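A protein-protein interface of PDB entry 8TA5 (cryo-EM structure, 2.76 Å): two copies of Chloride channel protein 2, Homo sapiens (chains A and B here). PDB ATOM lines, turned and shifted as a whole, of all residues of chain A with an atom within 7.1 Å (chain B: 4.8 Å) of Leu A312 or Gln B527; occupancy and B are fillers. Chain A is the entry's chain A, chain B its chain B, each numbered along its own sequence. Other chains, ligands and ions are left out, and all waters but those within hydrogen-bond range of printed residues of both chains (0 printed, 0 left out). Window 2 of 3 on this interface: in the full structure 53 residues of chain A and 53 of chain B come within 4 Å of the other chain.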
ATOM      1  N   PHE A 310      20.952 -15.977   4.914  1.00  0.00           N
ATOM      2  CA  PHE A 310      21.228 -16.998   3.914  1.00  0.00           C
ATOM      3  C   PHE A 310      20.347 -18.217   4.148  1.00  0.00           C
ATOM      4  O   PHE A 310      19.941 -18.504   5.278  1.00  0.00           O
ATOM      5  CB  PHE A 310      22.702 -17.415   3.936  1.00  0.00           C
ATOM      6  CG  PHE A 310      23.655 -16.290   3.665  1.00  0.00           C
ATOM      7  CD1 PHE A 310      23.409 -15.389   2.647  1.00  0.00           C
ATOM      8  CD2 PHE A 310      24.801 -16.138   4.425  1.00  0.00           C
ATOM      9  CE1 PHE A 310      24.284 -14.354   2.394  1.00  0.00           C
ATOM     10  CE2 PHE A 310      25.681 -15.105   4.177  1.00  0.00           C
ATOM     11  CZ  PHE A 310      25.421 -14.212   3.160  1.00  0.00           C
ATOM     12  N   ARG A 311      20.051 -18.930   3.065  1.00  0.00           N
ATOM     13  CA  ARG A 311      19.228 -20.126   3.161  1.00  0.00           C
ATOM     14  C   ARG A 311      19.965 -21.225   3.917  1.00  0.00           C
ATOM     15  O   ARG A 311      21.172 -21.420   3.750  1.00  0.00           O
ATOM     16  CB  ARG A 311      18.830 -20.610   1.766  1.00  0.00           C
ATOM     17  CG  ARG A 311      19.984 -21.108   0.915  1.00  0.00           C
ATOM     18  CD  ARG A 311      19.488 -21.891  -0.287  1.00  0.00           C
ATOM     19  NE  ARG A 311      20.587 -22.319  -1.144  1.00  0.00           N
ATOM     20  CZ  ARG A 311      20.975 -21.679  -2.237  1.00  0.00           C
ATOM     21  NH1 ARG A 311      20.376 -20.572  -2.640  1.00  0.00           N
ATOM     22  NH2 ARG A 311      21.991 -22.164  -2.945  1.00  0.00           N
ATOM     23  N   LEU A 312      19.232 -21.932   4.775  1.00  0.00           N
ATOM     24  CA  LEU A 312      19.801 -23.010   5.570  1.00  0.00           C
ATOM     25  C   LEU A 312      19.853 -24.339   4.830  1.00  0.00           C
ATOM     26  O   LEU A 312      20.529 -25.263   5.296  1.00  0.00           O
ATOM     27  CB  LEU A 312      19.006 -23.185   6.868  1.00  0.00           C
ATOM     28  CG  LEU A 312      19.503 -22.414   8.092  1.00  0.00           C
ATOM     29  CD1 LEU A 312      18.849 -22.944   9.356  1.00  0.00           C
ATOM     30  CD2 LEU A 312      21.017 -22.483   8.196  1.00  0.00           C
ATOM     31  N   ASP A 313      19.164 -24.460   3.698  1.00  0.00           N
ATOM     32  CA  ASP A 313      19.100 -25.705   2.943  1.00  0.00           C
ATOM     33  C   ASP A 313      20.086 -25.627   1.783  1.00  0.00           C
ATOM     34  O   ASP A 313      19.840 -24.925   0.797  1.00  0.00           O
ATOM     35  CB  ASP A 313      17.681 -25.962   2.442  1.00  0.00           C
ATOM     36  CG  ASP A 313      16.756 -26.446   3.540  1.00  0.00           C
ATOM     37  OD1 ASP A 313      17.124 -27.409   4.244  1.00  0.00           O
ATOM     38  OD2 ASP A 313      15.662 -25.866   3.699  1.00  0.00           O
ATOM     39  N   PHE A 314      21.191 -26.357   1.903  1.00  0.00           N
ATOM     40  CA  PHE A 314      22.234 -26.407   0.884  1.00  0.00           C
ATOM     41  C   PHE A 314      22.731 -25.012   0.491  1.00  0.00           C
ATOM     42  O   PHE A 314      22.563 -24.589  -0.657  1.00  0.00           O
ATOM     43  CB  PHE A 314      21.748 -27.168  -0.342  1.00  0.00           C
ATOM     44  CG  PHE A 314      21.907 -28.656  -0.234  1.00  0.00           C
ATOM     45  CD1 PHE A 314      23.162 -29.223  -0.092  1.00  0.00           C
ATOM     46  CD2 PHE A 314      20.801 -29.488  -0.272  1.00  0.00           C
ATOM     47  CE1 PHE A 314      23.311 -30.594   0.010  1.00  0.00           C
ATOM     48  CE2 PHE A 314      20.943 -30.859  -0.171  1.00  0.00           C
ATOM     49  CZ  PHE A 314      22.200 -31.412  -0.029  1.00  0.00           C
ATOM     50  N   PRO A 315      23.338 -24.272   1.423  1.00  0.00           N
ATOM     51  CA  PRO A 315      23.874 -22.951   1.058  1.00  0.00           C
ATOM     52  C   PRO A 315      24.981 -23.016   0.021  1.00  0.00           C
ATOM     53  O   PRO A 315      25.134 -22.075  -0.768  1.00  0.00           O
ATOM     54  CB  PRO A 315      24.377 -22.398   2.398  1.00  0.00           C
ATOM     55  CG  PRO A 315      24.687 -23.604   3.204  1.00  0.00           C
ATOM     56  CD  PRO A 315      23.677 -24.643   2.808  1.00  0.00           C
ATOM     57  N   GLY A 526      25.903 -13.735  12.562  1.00  0.00           N
ATOM     58  CA  GLY A 526      24.758 -14.359  13.187  1.00  0.00           C
ATOM     59  C   GLY A 526      24.354 -15.696  12.613  1.00  0.00           C
ATOM     60  O   GLY A 526      23.311 -16.231  13.009  1.00  0.00           O
ATOM     61  N   GLN A 527      25.138 -16.255  11.694  1.00  0.00           N
ATOM     62  CA  GLN A 527      24.857 -17.553  11.101  1.00  0.00           C
ATOM     63  C   GLN A 527      26.127 -18.389  11.089  1.00  0.00           C
ATOM     64  O   GLN A 527      27.240 -17.858  11.065  1.00  0.00           O
ATOM     65  CB  GLN A 527      24.307 -17.415   9.677  1.00  0.00           C
ATOM     66  CG  GLN A 527      22.975 -16.694   9.595  1.00  0.00           C
ATOM     67  CD  GLN A 527      22.200 -17.052   8.349  1.00  0.00           C
ATOM     68  OE1 GLN A 527      22.671 -16.844   7.232  1.00  0.00           O
ATOM     69  NE2 GLN A 527      21.004 -17.597   8.530  1.00  0.00           N
ATOM     70  N   ILE A 528      25.951 -19.710  11.102  1.00  0.00           N
ATOM     71  CA  ILE A 528      27.076 -20.634  11.192  1.00  0.00           C
ATOM     72  C   ILE A 528      26.982 -21.658  10.066  1.00  0.00           C
ATOM     73  O   ILE A 528      27.585 -22.735  10.129  1.00  0.00           O
ATOM     74  CB  ILE A 528      27.119 -21.296  12.586  1.00  0.00           C
ATOM     75  CG1 ILE A 528      28.509 -21.861  12.890  1.00  0.00           C
ATOM     76  CG2 ILE A 528      26.035 -22.353  12.729  1.00  0.00           C
ATOM     77  CD1 ILE A 528      28.778 -22.046  14.363  1.00  0.00           C
ATOM     78  N   ALA A 529      26.247 -21.311   9.007  1.00  0.00           N
ATOM     79  CA  ALA A 529      26.057 -22.244   7.899  1.00  0.00           C
ATOM     80  C   ALA A 529      27.353 -22.460   7.124  1.00  0.00           C
ATOM     81  O   ALA A 529      27.724 -23.601   6.823  1.00  0.00           O
ATOM     82  CB  ALA A 529      24.954 -21.735   6.974  1.00  0.00           C
ATOM     83  N   LYS B 307      19.916 -30.543  13.560  1.00  0.00           N
ATOM     84  CA  LYS B 307      19.632 -29.217  13.024  1.00  0.00           C
ATOM     85  C   LYS B 307      18.281 -28.694  13.496  1.00  0.00           C
ATOM     86  O   LYS B 307      17.279 -29.413  13.484  1.00  0.00           O
ATOM     87  CB  LYS B 307      19.667 -29.269  11.496  1.00  0.00           C
ATOM     88  CG  LYS B 307      19.541 -27.918  10.812  1.00  0.00           C
ATOM     89  CD  LYS B 307      20.831 -27.536  10.106  1.00  0.00           C
ATOM     90  CE  LYS B 307      20.916 -26.037   9.881  1.00  0.00           C
ATOM     91  NZ  LYS B 307      22.250 -25.633   9.356  1.00  0.00           N
ATOM     92  N   THR B 308      18.267 -27.432  13.920  1.00  0.00           N
ATOM     93  CA  THR B 308      17.063 -26.737  14.344  1.00  0.00           C
ATOM     94  C   THR B 308      16.676 -25.688  13.309  1.00  0.00           C
ATOM     95  O   THR B 308      17.501 -25.236  12.511  1.00  0.00           O
ATOM     96  CB  THR B 308      17.260 -26.072  15.711  1.00  0.00           C
ATOM     97  OG1 THR B 308      18.412 -25.221  15.670  1.00  0.00           O
ATOM     98  CG2 THR B 308      17.452 -27.122  16.794  1.00  0.00           C
ATOM     99  N   ARG B 309      15.402 -25.300  13.331  1.00  0.00           N
ATOM    100  CA  ARG B 309      14.845 -24.342  12.379  1.00  0.00           C
ATOM    101  C   ARG B 309      14.088 -23.239  13.109  1.00  0.00           C
ATOM    102  O   ARG B 309      12.959 -22.889  12.760  1.00  0.00           O
ATOM    103  CB  ARG B 309      13.931 -25.027  11.365  1.00  0.00           C
ATOM    104  CG  ARG B 309      14.166 -26.516  11.199  1.00  0.00           C
ATOM    105  CD  ARG B 309      15.354 -26.780  10.291  1.00  0.00           C
ATOM    106  NE  ARG B 309      15.165 -26.209   8.964  1.00  0.00           N
ATOM    107  CZ  ARG B 309      16.076 -26.235   8.000  1.00  0.00           C
ATOM    108  NH1 ARG B 309      17.264 -26.786   8.187  1.00  0.00           N
ATOM    109  NH2 ARG B 309      15.789 -25.691   6.821  1.00  0.00           N
ATOM    110  N   PHE B 310      14.706 -22.677  14.144  1.00  0.00           N
ATOM    111  CA  PHE B 310      14.098 -21.564  14.858  1.00  0.00           C
ATOM    112  C   PHE B 310      14.079 -20.312  13.988  1.00  0.00           C
ATOM    113  O   PHE B 310      14.915 -20.133  13.097  1.00  0.00           O
ATOM    114  CB  PHE B 310      14.852 -21.277  16.156  1.00  0.00           C
ATOM    115  CG  PHE B 310      14.919 -22.449  17.091  1.00  0.00           C
ATOM    116  CD1 PHE B 310      13.827 -23.280  17.261  1.00  0.00           C
ATOM    117  CD2 PHE B 310      16.074 -22.713  17.807  1.00  0.00           C
ATOM    118  CE1 PHE B 310      13.887 -24.355  18.122  1.00  0.00           C
ATOM    119  CE2 PHE B 310      16.140 -23.785  18.669  1.00  0.00           C
ATOM    120  CZ  PHE B 310      15.044 -24.608  18.827  1.00  0.00           C
ATOM    121  N   PHE B 522      26.340 -25.070  19.463  1.00  0.00           N
ATOM    122  CA  PHE B 522      26.150 -24.233  18.281  1.00  0.00           C
ATOM    123  C   PHE B 522      26.491 -24.993  17.005  1.00  0.00           C
ATOM    124  O   PHE B 522      25.798 -24.852  15.989  1.00  0.00           O
ATOM    125  CB  PHE B 522      26.984 -22.958  18.386  1.00  0.00           C
ATOM    126  CG  PHE B 522      26.560 -22.054  19.501  1.00  0.00           C
ATOM    127  CD1 PHE B 522      25.240 -22.019  19.917  1.00  0.00           C
ATOM    128  CD2 PHE B 522      27.480 -21.235  20.134  1.00  0.00           C
ATOM    129  CE1 PHE B 522      24.847 -21.192  20.945  1.00  0.00           C
ATOM    130  CE2 PHE B 522      27.091 -20.407  21.163  1.00  0.00           C
ATOM    131  CZ  PHE B 522      25.775 -20.386  21.569  1.00  0.00           C
ATOM    132  N   THR B 525      23.517 -27.842  16.612  1.00  0.00           N
ATOM    133  CA  THR B 525      22.200 -27.434  16.140  1.00  0.00           C
ATOM    134  C   THR B 525      22.238 -26.673  14.823  1.00  0.00           C
ATOM    135  O   THR B 525      21.193 -26.529  14.179  1.00  0.00           O
ATOM    136  CB  THR B 525      21.503 -26.570  17.196  1.00  0.00           C
ATOM    137  OG1 THR B 525      22.332 -25.448  17.521  1.00  0.00           O
ATOM    138  CG2 THR B 525      21.239 -27.380  18.454  1.00  0.00           C
ATOM    139  N   GLY B 526      23.404 -26.189  14.403  1.00  0.00           N
ATOM    140  CA  GLY B 526      23.503 -25.446  13.166  1.00  0.00           C
ATOM    141  C   GLY B 526      23.021 -24.015  13.233  1.00  0.00           C
ATOM    142  O   GLY B 526      22.924 -23.364  12.187  1.00  0.00           O
ATOM    143  N   GLN B 527      22.716 -23.504  14.423  1.00  0.00           N
ATOM    144  CA  GLN B 527      22.244 -22.139  14.590  1.00  0.00           C
ATOM    145  C   GLN B 527      22.932 -21.511  15.791  1.00  0.00           C
ATOM    146  O   GLN B 527      23.320 -22.203  16.735  1.00  0.00           O
ATOM    147  CB  GLN B 527      20.722 -22.086  14.769  1.00  0.00           C
ATOM    148  CG  GLN B 527      19.937 -22.385  13.506  1.00  0.00           C
ATOM    149  CD  GLN B 527      18.505 -21.905  13.587  1.00  0.00           C
ATOM    150  OE1 GLN B 527      17.792 -22.206  14.542  1.00  0.00           O
ATOM    151  NE2 GLN B 527      18.076 -21.148  12.587  1.00  0.00           N
ATOM    152  N   ILE B 528      23.080 -20.188  15.747  1.00  0.00           N
ATOM    153  CA  ILE B 528      23.769 -19.454  16.803  1.00  0.00           C
ATOM    154  C   ILE B 528      22.873 -18.316  17.286  1.00  0.00           C
ATOM    155  O   ILE B 528      23.346 -17.312  17.832  1.00  0.00           O
ATOM    156  CB  ILE B 528      25.142 -18.957  16.303  1.00  0.00           C
ATOM    157  CG1 ILE B 528      26.063 -18.592  17.471  1.00  0.00           C
ATOM    158  CG2 ILE B 528      24.993 -17.808  15.318  1.00  0.00           C
ATOM    159  CD1 ILE B 528      27.496 -18.353  17.058  1.00  0.00           C
ATOM    160  N   ALA B 529      21.560 -18.485  17.122  1.00  0.00           N
ATOM    161  CA  ALA B 529      20.620 -17.421  17.458  1.00  0.00           C
ATOM    162  C   ALA B 529      20.439 -17.246  18.961  1.00  0.00           C
ATOM    163  O   ALA B 529      20.067 -16.156  19.410  1.00  0.00           O
ATOM    164  CB  ALA B 529      19.266 -17.694  16.801  1.00  0.00           C
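Of the printed residues of chain B, Leu A312 touches Lys B307 and Gln B527. Gln B527 touches just these residues of chain A: Leu A312 and Ile A528. Gly B526 touches just one residue of chain A: Ile A528 (3.3 Å). Of the printed residues of chain B, Gly A526 touches Ile B528 (3.3 Å). Printed residues of chain A within 4 Å of Ile B528: Gly A526 and Gln A527. Of the printed residues of chain A, Arg B309 touches Asp A313. Of the printed residues of chain B, Asp A313 touches Arg B309 (3.1 Å). Printed residues of chain B within 4 Å of Gln A527: Ile B528. Arg A311 touches none of the printed residues of chain B. Pro A315 touches none of the printed residues of chain B. The nearest residue of chain A that does not touch Gln B527 is Gly A526 (6.0 Å).
Among the printed residues, merely in contact across the chains: Leu A312 with Lys B307, Leu A312 with Gln B527, Gly A526 with Ile B528, Gln A527 with Ile B528, Ile A528 with Gly B526 and Ile A528 with Gln B527.
Gly A526 touches Ile B528, and with the chains exchanged Ile A528 touches Gly B526. Gln A527 touches Ile B528, and with the chains exchanged Ile A528 touches Gln B527.
Of the 10 printed residues of chain B, 5 touch a printed residue of chain A. Of the 10 printed residues of chain A, 5 touch a printed residue of chain B. Hydrophobic or aromatic side chains of chain A that line the printed part of chain B: Leu A312 and Ile A528. Among the printed residues, Asp or Glu carboxylates within 4 Å of a Lys or Arg side-chain nitrogen of the other chain: Asp A313 with Arg B309.
The backbone NH (N) of Phe A310 is in hydrogen-bond range of the side-chain amide oxygen (OE1) of Gln A527, at 3.0 Å. The backbone carbonyl oxygen of Asp A313 lies close to the guanidinium group of Arg A311 (3.3 Å). OE1 of Gln B527 is in hydrogen-bond range of OG1 of Thr B308 (3.3 Å). The backbone NH (N) of Phe B310 is in hydrogen-bond range of the side-chain amide oxygen (OE1) of Gln B527 (3.1 Å). O of Gln B527 is in hydrogen-bond range of OG1 of Thr B525.
The side-chain carboxylate (OD2) of Asp A313 lies within salt-bridge range of the guanidinium group (NH2) of Arg B309 (3.1 Å).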
